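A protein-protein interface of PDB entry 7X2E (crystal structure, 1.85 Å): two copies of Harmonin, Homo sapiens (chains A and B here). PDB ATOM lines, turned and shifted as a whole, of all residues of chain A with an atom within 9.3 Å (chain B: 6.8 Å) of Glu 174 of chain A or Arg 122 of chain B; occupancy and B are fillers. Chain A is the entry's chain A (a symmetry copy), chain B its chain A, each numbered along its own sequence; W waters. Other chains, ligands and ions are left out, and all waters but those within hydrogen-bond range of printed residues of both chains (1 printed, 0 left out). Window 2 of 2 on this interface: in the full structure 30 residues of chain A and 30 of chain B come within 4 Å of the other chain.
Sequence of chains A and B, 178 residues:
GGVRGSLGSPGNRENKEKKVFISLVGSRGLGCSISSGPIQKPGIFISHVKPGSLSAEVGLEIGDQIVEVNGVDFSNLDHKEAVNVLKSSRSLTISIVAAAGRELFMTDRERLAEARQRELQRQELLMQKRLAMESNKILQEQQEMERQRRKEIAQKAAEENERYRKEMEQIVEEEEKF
OE2 of Glu 119 of chain B lies close to OE2 of Glu 175 of chain A (2.6 Å). The guanidinium group (NE) of Arg 122 of chain B is in salt-bridge range of the side-chain carboxylate (OE1) of Glu 175 of chain A.
OE1 of Glu 119 of chain B lies within salt-bridge range of NH2 of Arg 122 of chain B, 2.9 Å away. The side-chain amide nitrogen (NE2) of Gln 123 of chain B lies within hydrogen-bond range of the side-chain carboxylate (OE2) of Glu 119 of chain B (2.8 Å).
Among the printed residues, pairs that only touch across the chains: Ile 171 of chain A with Leu 125 of chain B (3.8 Å), Ile 171 of chain A with Leu 126 of chain B (3.8 Å), Met 168 of chain A with Leu 126 of chain B (3.8 Å), Ile 171 of chain A with Arg 122 of chain B (3.9 Å) and Glu 174 of chain A with Arg 122 of chain B (3.99 Å).
Of the printed residues of chain B, Met 168 of chain A touches Leu 126 (3.8 Å). Printed residues of chain B within 4 Å of Ile 171 of chain A: Arg 122, Leu 125 and Leu 126. Printed residues of chain B within 4 Å of Glu 174 of chain A: Arg 122 (3.99 Å). Of the printed residues of chain B, Glu 175 of chain A touches Glu 119 (2.6 Å) and Arg 122 (2.9 Å). Phe 178 of chain A touches none of the printed residues of chain B. Of the printed residues of chain A, Arg 122 of chain B touches Ile 171, Glu 174 and Glu 175. No residue of chain A comes within 4 Å of Glu 124 of chain B. Of the printed residues of chain A, Leu 125 of chain B touches Ile 171. Printed residues of chain A within 4 Å of Leu 126 of chain B: Met 168 and Ile 171. The nearest printed residue of chain A that does not touch Arg 122 of chain B is Lys 177 of chain A (5.9 Å). The nearest printed residue of chain A that does not touch Leu 126 of chain B is Val 172 of chain A (4.4 Å).
Of the 13 printed residues of chain B, 4 touch a printed residue of chain A. Printed residues of chain B that touch a printed residue of chain A: Glu 119, Arg 122, Leu 125 and Leu 126. Hydrophobic or aromatic side chains of chain B that line the printed part of chain A: Leu 125 and Leu 126. Along chain A the printed residues that touch a printed residue of chain B span positions 168 to 175. Among the printed residues, 7 pairs touch across the chains. Among the printed residues, Asp or Glu carboxylates within 4 Å of a Lys or Arg side-chain nitrogen of the other chain: Glu 175 of chain A with Arg 122 of chain B.
No position is printed for both chains. Of the 7 pairs that touch across the chains among the printed residues, none has its exchanged pair printed and touching as well.
Water W1 lies within hydrogen-bond range of the guanidinium group (NH1) of Arg 122 of chain B (2.7 Å) and the side-chain carboxylate (OE2) of Glu 174 of chain A (3.1 Å).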
ATOM      1  N   GLU A 167      13.442  22.903 -18.210  1.00  0.00           N
ATOM      2  CA  GLU A 167      12.801  23.139 -19.502  1.00  0.00           C
ATOM      3  C   GLU A 167      11.822  22.021 -19.852  1.00  0.00           C
ATOM      4  O   GLU A 167      10.721  22.291 -20.349  1.00  0.00           O
ATOM      5  CB  GLU A 167      13.860  23.315 -20.596  1.00  0.00           C
ATOM      6  CG  GLU A 167      14.696  24.583 -20.424  1.00  0.00           C
ATOM      7  CD  GLU A 167      15.928  24.613 -21.302  1.00  0.00           C
ATOM      8  OE1 GLU A 167      16.295  23.553 -21.847  1.00  0.00           O
ATOM      9  OE2 GLU A 167      16.539  25.694 -21.430  1.00  0.00           O
ATOM     10  N   MET A 168      12.189  20.764 -19.582  1.00  0.00           N
ATOM     11  CA  MET A 168      11.262  19.657 -19.820  1.00  0.00           C
ATOM     12  C   MET A 168      10.046  19.739 -18.904  1.00  0.00           C
ATOM     13  O   MET A 168       8.924  19.439 -19.329  1.00  0.00           O
ATOM     14  CB  MET A 168      11.973  18.317 -19.639  1.00  0.00           C
ATOM     15  CG  MET A 168      13.089  18.075 -20.637  1.00  0.00           C
ATOM     16  SD  MET A 168      13.951  16.498 -20.462  1.00  0.00           S
ATOM     17  CE  MET A 168      12.648  15.340 -20.875  1.00  0.00           C
ATOM     18  N   GLU A 169      10.246  20.123 -17.639  1.00  0.00           N
ATOM     19  CA  GLU A 169       9.107  20.291 -16.738  1.00  0.00           C
ATOM     20  C   GLU A 169       8.167  21.386 -17.230  1.00  0.00           C
ATOM     21  O   GLU A 169       6.943  21.278 -17.081  1.00  0.00           O
ATOM     22  CB  GLU A 169       9.592  20.589 -15.316  1.00  0.00           C
ATOM     23  CG  GLU A 169      10.484  19.501 -14.726  1.00  0.00           C
ATOM     24  CD  GLU A 169      10.985  19.833 -13.329  1.00  0.00           C
ATOM     25  OE1 GLU A 169      11.242  18.894 -12.547  1.00  0.00           O
ATOM     26  OE2 GLU A 169      11.126  21.033 -13.018  1.00  0.00           O
ATOM     27  N   GLN A 170       8.716  22.440 -17.836  1.00  0.00           N
ATOM     28  CA  GLN A 170       7.869  23.490 -18.392  1.00  0.00           C
ATOM     29  C   GLN A 170       7.056  22.975 -19.575  1.00  0.00           C
ATOM     30  O   GLN A 170       5.872  23.306 -19.712  1.00  0.00           O
ATOM     31  CB  GLN A 170       8.726  24.690 -18.795  1.00  0.00           C
ATOM     32  CG  GLN A 170       9.253  25.481 -17.605  1.00  0.00           C
ATOM     33  CD  GLN A 170      10.410  26.393 -17.964  1.00  0.00           C
ATOM     34  OE1 GLN A 170      10.811  26.482 -19.124  1.00  0.00           O
ATOM     35  NE2 GLN A 170      10.953  27.079 -16.963  1.00  0.00           N
ATOM     36  N   ILE A 171       7.667  22.160 -20.437  1.00  0.00           N
ATOM     37  CA  ILE A 171       6.928  21.577 -21.553  1.00  0.00           C
ATOM     38  C   ILE A 171       5.876  20.602 -21.041  1.00  0.00           C
ATOM     39  O   ILE A 171       4.765  20.523 -21.580  1.00  0.00           O
ATOM     40  CB  ILE A 171       7.895  20.899 -22.543  1.00  0.00           C
ATOM     41  CG1 ILE A 171       8.893  21.915 -23.099  1.00  0.00           C
ATOM     42  CG2 ILE A 171       7.120  20.239 -23.689  1.00  0.00           C
ATOM     43  CD1 ILE A 171      10.185  21.294 -23.581  1.00  0.00           C
ATOM     44  N   VAL A 172       6.200  19.860 -19.976  1.00  0.00           N
ATOM     45  CA  VAL A 172       5.248  18.912 -19.401  1.00  0.00           C
ATOM     46  C   VAL A 172       4.018  19.642 -18.870  1.00  0.00           C
ATOM     47  O   VAL A 172       2.891  19.137 -18.957  1.00  0.00           O
ATOM     48  CB  VAL A 172       5.938  18.071 -18.311  1.00  0.00           C
ATOM     49  CG1 VAL A 172       4.913  17.423 -17.391  1.00  0.00           C
ATOM     50  CG2 VAL A 172       6.826  17.011 -18.954  1.00  0.00           C
ATOM     51  N   GLU A 173       4.214  20.843 -18.318  1.00  0.00           N
ATOM     52  CA  GLU A 173       3.080  21.670 -17.915  1.00  0.00           C
ATOM     53  C   GLU A 173       2.158  21.952 -19.096  1.00  0.00           C
ATOM     54  O   GLU A 173       0.928  21.907 -18.960  1.00  0.00           O
ATOM     55  CB  GLU A 173       3.581  22.978 -17.300  1.00  0.00           C
ATOM     56  CG  GLU A 173       4.231  22.810 -15.934  1.00  0.00           C
ATOM     57  CD  GLU A 173       4.683  24.130 -15.336  1.00  0.00           C
ATOM     58  OE1 GLU A 173       5.692  24.139 -14.598  1.00  0.00           O
ATOM     59  OE2 GLU A 173       4.029  25.159 -15.607  1.00  0.00           O
ATOM     60  N   GLU A 174       2.733  22.247 -20.266  1.00  0.00           N
ATOM     61  CA  GLU A 174       1.924  22.430 -21.467  1.00  0.00           C
ATOM     62  C   GLU A 174       1.304  21.112 -21.916  1.00  0.00           C
ATOM     63  O   GLU A 174       0.155  21.081 -22.370  1.00  0.00           O
ATOM     64  CB  GLU A 174       2.777  23.022 -22.588  1.00  0.00           C
ATOM     65  CG  GLU A 174       3.115  24.490 -22.411  1.00  0.00           C
ATOM     66  CD  GLU A 174       4.105  24.983 -23.447  1.00  0.00           C
ATOM     67  OE1 GLU A 174       4.574  26.134 -23.323  1.00  0.00           O
ATOM     68  OE2 GLU A 174       4.410  24.218 -24.389  1.00  0.00           O
ATOM     69  N   GLU A 175       2.060  20.017 -21.802  1.00  0.00           N
ATOM     70  CA  GLU A 175       1.540  18.693 -22.128  1.00  0.00           C
ATOM     71  C   GLU A 175       0.316  18.340 -21.293  1.00  0.00           C
ATOM     72  O   GLU A 175      -0.600  17.666 -21.782  1.00  0.00           O
ATOM     73  CB  GLU A 175       2.640  17.650 -21.918  1.00  0.00           C
ATOM     74  CG  GLU A 175       2.291  16.240 -22.359  1.00  0.00           C
ATOM     75  CD  GLU A 175       2.317  16.055 -23.864  1.00  0.00           C
ATOM     76  OE1 GLU A 175       2.728  16.984 -24.593  1.00  0.00           O
ATOM     77  OE2 GLU A 175       1.936  14.958 -24.314  1.00  0.00           O
ATOM     78  N   GLU A 176       0.275  18.789 -20.041  1.00  0.00           N
ATOM     79  CA  GLU A 176      -0.784  18.424 -19.109  1.00  0.00           C
ATOM     80  C   GLU A 176      -1.988  19.354 -19.184  1.00  0.00           C
ATOM     81  O   GLU A 176      -2.835  19.328 -18.285  1.00  0.00           O
ATOM     82  CB  GLU A 176      -0.229  18.383 -17.685  1.00  0.00           C
ATOM     83  CG  GLU A 176       0.628  17.155 -17.415  1.00  0.00           C
ATOM     84  CD  GLU A 176       0.727  16.819 -15.943  1.00  0.00           C
ATOM     85  OE1 GLU A 176       1.374  17.589 -15.203  1.00  0.00           O
ATOM     86  OE2 GLU A 176       0.155  15.788 -15.527  1.00  0.00           O
ATOM     87  N   LYS A 177      -2.080  20.178 -20.224  1.00  0.00           N
ATOM     88  CA  LYS A 177      -3.308  20.899 -20.533  1.00  0.00           C
ATOM     89  C   LYS A 177      -4.111  20.045 -21.507  1.00  0.00           C
ATOM     90  O   LYS A 177      -3.688  19.822 -22.646  1.00  0.00           O
ATOM     91  CB  LYS A 177      -3.006  22.280 -21.107  1.00  0.00           C
ATOM     92  CG  LYS A 177      -2.030  23.076 -20.262  1.00  0.00           C
ATOM     93  CD  LYS A 177      -1.801  24.461 -20.828  1.00  0.00           C
ATOM     94  CE  LYS A 177      -1.602  25.459 -19.701  1.00  0.00           C
ATOM     95  NZ  LYS A 177      -2.642  25.288 -18.648  1.00  0.00           N
ATOM     96  N   PHE A 178      -5.253  19.549 -21.049  1.00  0.00           N
ATOM     97  CA  PHE A 178      -6.034  18.596 -21.827  1.00  0.00           C
ATOM     98  C   PHE A 178      -7.221  19.264 -22.510  1.00  0.00           C
ATOM     99  O   PHE A 178      -7.669  20.337 -22.107  1.00  0.00           O
ATOM    100  CB  PHE A 178      -6.501  17.454 -20.927  1.00  0.00           C
ATOM    101  CG  PHE A 178      -5.373  16.699 -20.283  1.00  0.00           C
ATOM    102  CD1 PHE A 178      -4.565  15.858 -21.035  1.00  0.00           C
ATOM    103  CD2 PHE A 178      -5.104  16.847 -18.933  1.00  0.00           C
ATOM    104  CE1 PHE A 178      -3.521  15.167 -20.446  1.00  0.00           C
ATOM    105  CE2 PHE A 178      -4.061  16.160 -18.339  1.00  0.00           C
ATOM    106  CZ  PHE A 178      -3.268  15.320 -19.098  1.00  0.00           C
ATOM    107  OXT PHE A 178      -7.752  18.745 -23.494  1.00  0.00           O
ATOM    108  N   ALA B 115      -4.067  19.523 -33.755  1.00  0.00           N
ATOM    109  CA  ALA B 115      -3.723  18.898 -32.482  1.00  0.00           C
ATOM    110  C   ALA B 115      -2.468  18.044 -32.610  1.00  0.00           C
ATOM    111  O   ALA B 115      -1.600  18.067 -31.728  1.00  0.00           O
ATOM    112  CB  ALA B 115      -4.896  18.056 -31.978  1.00  0.00           C
ATOM    113  N   ARG B 116      -2.361  17.276 -33.696  1.00  0.00           N
ATOM    114  CA  ARG B 116      -1.154  16.490 -33.934  1.00  0.00           C
ATOM    115  C   ARG B 116       0.079  17.379 -34.015  1.00  0.00           C
ATOM    116  O   ARG B 116       1.127  17.053 -33.446  1.00  0.00           O
ATOM    117  CB  ARG B 116      -1.288  15.677 -35.222  1.00  0.00           C
ATOM    118  CG  ARG B 116      -0.080  14.782 -35.489  1.00  0.00           C
ATOM    119  CD  ARG B 116      -0.192  13.984 -36.786  1.00  0.00           C
ATOM    120  NE  ARG B 116      -1.391  13.159 -36.886  1.00  0.00           N
ATOM    121  CZ  ARG B 116      -1.438  11.871 -36.560  1.00  0.00           C
ATOM    122  NH1 ARG B 116      -0.354  11.262 -36.100  1.00  0.00           N
ATOM    123  NH2 ARG B 116      -2.569  11.190 -36.692  1.00  0.00           N
ATOM    124  N   GLN B 117      -0.018  18.498 -34.739  1.00  0.00           N
ATOM    125  CA  GLN B 117       1.148  19.358 -34.917  1.00  0.00           C
ATOM    126  C   GLN B 117       1.597  19.965 -33.594  1.00  0.00           C
ATOM    127  O   GLN B 117       2.799  20.045 -33.318  1.00  0.00           O
ATOM    128  CB  GLN B 117       0.844  20.460 -35.934  1.00  0.00           C
ATOM    129  CG  GLN B 117       1.031  20.042 -37.386  1.00  0.00           C
ATOM    130  CD  GLN B 117       2.320  19.273 -37.622  1.00  0.00           C
ATOM    131  OE1 GLN B 117       3.415  19.817 -37.486  1.00  0.00           O
ATOM    132  NE2 GLN B 117       2.193  18.000 -37.987  1.00  0.00           N
ATOM    133  N   ARG B 118       0.647  20.395 -32.760  1.00  0.00           N
ATOM    134  CA  ARG B 118       1.013  20.966 -31.467  1.00  0.00           C
ATOM    135  C   ARG B 118       1.682  19.921 -30.581  1.00  0.00           C
ATOM    136  O   ARG B 118       2.666  20.215 -29.892  1.00  0.00           O
ATOM    137  CB  ARG B 118      -0.224  21.540 -30.780  1.00  0.00           C
ATOM    138  CG  ARG B 118      -0.694  22.870 -31.353  1.00  0.00           C
ATOM    139  CD  ARG B 118      -1.852  23.428 -30.539  1.00  0.00           C
ATOM    140  NE  ARG B 118      -2.999  22.524 -30.564  1.00  0.00           N
ATOM    141  CZ  ARG B 118      -4.196  22.844 -31.044  1.00  0.00           C
ATOM    142  NH1 ARG B 118      -4.412  24.054 -31.541  1.00  0.00           N
ATOM    143  NH2 ARG B 118      -5.179  21.950 -31.027  1.00  0.00           N
ATOM    144  N   GLU B 119       1.161  18.692 -30.591  1.00  0.00           N
ATOM    145  CA  GLU B 119       1.777  17.617 -29.820  1.00  0.00           C
ATOM    146  C   GLU B 119       3.164  17.280 -30.357  1.00  0.00           C
ATOM    147  O   GLU B 119       4.095  17.040 -29.577  1.00  0.00           O
ATOM    148  CB  GLU B 119       0.873  16.385 -29.835  1.00  0.00           C
ATOM    149  CG  GLU B 119       1.405  15.179 -29.068  1.00  0.00           C
ATOM    150  CD  GLU B 119       1.373  15.350 -27.565  1.00  0.00           C
ATOM    151  OE1 GLU B 119       0.551  16.145 -27.055  1.00  0.00           O
ATOM    152  OE2 GLU B 119       2.166  14.666 -26.889  1.00  0.00           O
ATOM    153  N   LEU B 120       3.326  17.273 -31.683  1.00  0.00           N
ATOM    154  CA  LEU B 120       4.622  16.950 -32.275  1.00  0.00           C
ATOM    155  C   LEU B 120       5.675  17.983 -31.901  1.00  0.00           C
ATOM    156  O   LEU B 120       6.846  17.639 -31.691  1.00  0.00           O
ATOM    157  CB  LEU B 120       4.495  16.847 -33.796  1.00  0.00           C
ATOM    158  CG  LEU B 120       3.982  15.521 -34.363  1.00  0.00           C
ATOM    159  CD1 LEU B 120       3.795  15.617 -35.872  1.00  0.00           C
ATOM    160  CD2 LEU B 120       4.929  14.383 -34.006  1.00  0.00           C
ATOM    161  N   GLN B 121       5.282  19.256 -31.820  1.00  0.00           N
ATOM    162  CA  GLN B 121       6.230  20.301 -31.442  1.00  0.00           C
ATOM    163  C   GLN B 121       6.710  20.120 -30.007  1.00  0.00           C
ATOM    164  O   GLN B 121       7.907  20.258 -29.726  1.00  0.00           O
ATOM    165  CB  GLN B 121       5.595  21.678 -31.634  1.00  0.00           C
ATOM    166  CG  GLN B 121       5.363  22.023 -33.097  1.00  0.00           C
ATOM    167  CD  GLN B 121       4.415  23.187 -33.293  1.00  0.00           C
ATOM    168  OE1 GLN B 121       4.066  23.888 -32.343  1.00  0.00           O
ATOM    169  NE2 GLN B 121       3.998  23.406 -34.535  1.00  0.00           N
ATOM    170  N   ARG B 122       5.793  19.816 -29.084  1.00  0.00           N
ATOM    171  CA  ARG B 122       6.202  19.515 -27.716  1.00  0.00           C
ATOM    172  C   ARG B 122       7.083  18.273 -27.667  1.00  0.00           C
ATOM    173  O   ARG B 122       8.095  18.249 -26.955  1.00  0.00           O
ATOM    174  CB  ARG B 122       4.977  19.325 -26.821  1.00  0.00           C
ATOM    175  CG  ARG B 122       4.181  20.595 -26.549  1.00  0.00           C
ATOM    176  CD  ARG B 122       3.090  20.338 -25.521  1.00  0.00           C
ATOM    177  NE  ARG B 122       2.040  19.462 -26.036  1.00  0.00           N
ATOM    178  CZ  ARG B 122       0.950  19.887 -26.666  1.00  0.00           C
ATOM    179  NH1 ARG B 122       0.756  21.184 -26.862  1.00  0.00           N
ATOM    180  NH2 ARG B 122       0.050  19.013 -27.097  1.00  0.00           N
ATOM    181  N   GLN B 123       6.714  17.233 -28.423  1.00  0.00           N
ATOM    182  CA  GLN B 123       7.451  15.973 -28.380  1.00  0.00           C
ATOM    183  C   GLN B 123       8.838  16.113 -28.994  1.00  0.00           C
ATOM    184  O   GLN B 123       9.789  15.469 -28.536  1.00  0.00           O
ATOM    185  CB  GLN B 123       6.655  14.878 -29.092  1.00  0.00           C
ATOM    186  CG  GLN B 123       5.436  14.421 -28.296  1.00  0.00           C
ATOM    187  CD  GLN B 123       4.766  13.201 -28.892  1.00  0.00           C
ATOM    188  OE1 GLN B 123       5.183  12.696 -29.934  1.00  0.00           O
ATOM    189  NE2 GLN B 123       3.717  12.722 -28.231  1.00  0.00           N
ATOM    190  N   GLU B 124       8.974  16.943 -30.029  1.00  0.00           N
ATOM    191  CA  GLU B 124      10.297  17.190 -30.596  1.00  0.00           C
ATOM    192  C   GLU B 124      11.233  17.798 -29.557  1.00  0.00           C
ATOM    193  O   GLU B 124      12.393  17.385 -29.435  1.00  0.00           O
ATOM    194  CB  GLU B 124      10.181  18.104 -31.815  1.00  0.00           C
ATOM    195  N   LEU B 125      10.739  18.776 -28.793  1.00  0.00           N
ATOM    196  CA  LEU B 125      11.557  19.409 -27.761  1.00  0.00           C
ATOM    197  C   LEU B 125      11.855  18.448 -26.620  1.00  0.00           C
ATOM    198  O   LEU B 125      12.982  18.409 -26.110  1.00  0.00           O
ATOM    199  CB  LEU B 125      10.854  20.655 -27.224  1.00  0.00           C
ATOM    200  CG  LEU B 125      10.661  21.812 -28.197  1.00  0.00           C
ATOM    201  CD1 LEU B 125       9.920  22.949 -27.512  1.00  0.00           C
ATOM    202  CD2 LEU B 125      12.005  22.289 -28.740  1.00  0.00           C
ATOM    203  N   LEU B 126      10.851  17.678 -26.192  1.00  0.00           N
ATOM    204  CA  LEU B 126      11.071  16.703 -25.131  1.00  0.00           C
ATOM    205  C   LEU B 126      12.132  15.690 -25.531  1.00  0.00           C
ATOM    206  O   LEU B 126      12.968  15.296 -24.711  1.00  0.00           O
ATOM    207  CB  LEU B 126       9.762  15.999 -24.779  1.00  0.00           C
ATOM    208  CG  LEU B 126       8.765  16.830 -23.971  1.00  0.00           C
ATOM    209  CD1 LEU B 126       7.408  16.146 -23.918  1.00  0.00           C
ATOM    210  CD2 LEU B 126       9.304  17.084 -22.570  1.00  0.00           C
ATOM    211  N   MET B 127      12.132  15.264 -26.793  1.00  0.00           N
ATOM    212  CA  MET B 127      13.102  14.252 -27.184  1.00  0.00           C
ATOM    213  C   MET B 127      14.492  14.868 -27.276  1.00  0.00           C
ATOM    214  O   MET B 127      15.483  14.259 -26.857  1.00  0.00           O
ATOM    215  CB  MET B 127      12.697  13.619 -28.515  1.00  0.00           C
ATOM    216  CG  MET B 127      13.780  12.768 -29.153  1.00  0.00           C
ATOM    217  SD  MET B 127      13.838  11.216 -28.222  1.00  0.00           S
ATOM    218  CE  MET B 127      12.353  10.437 -28.844  1.00  0.00           C
HETATM  219  O   HOH W   1       2.260  23.409 -26.426  1.00  0.00           O
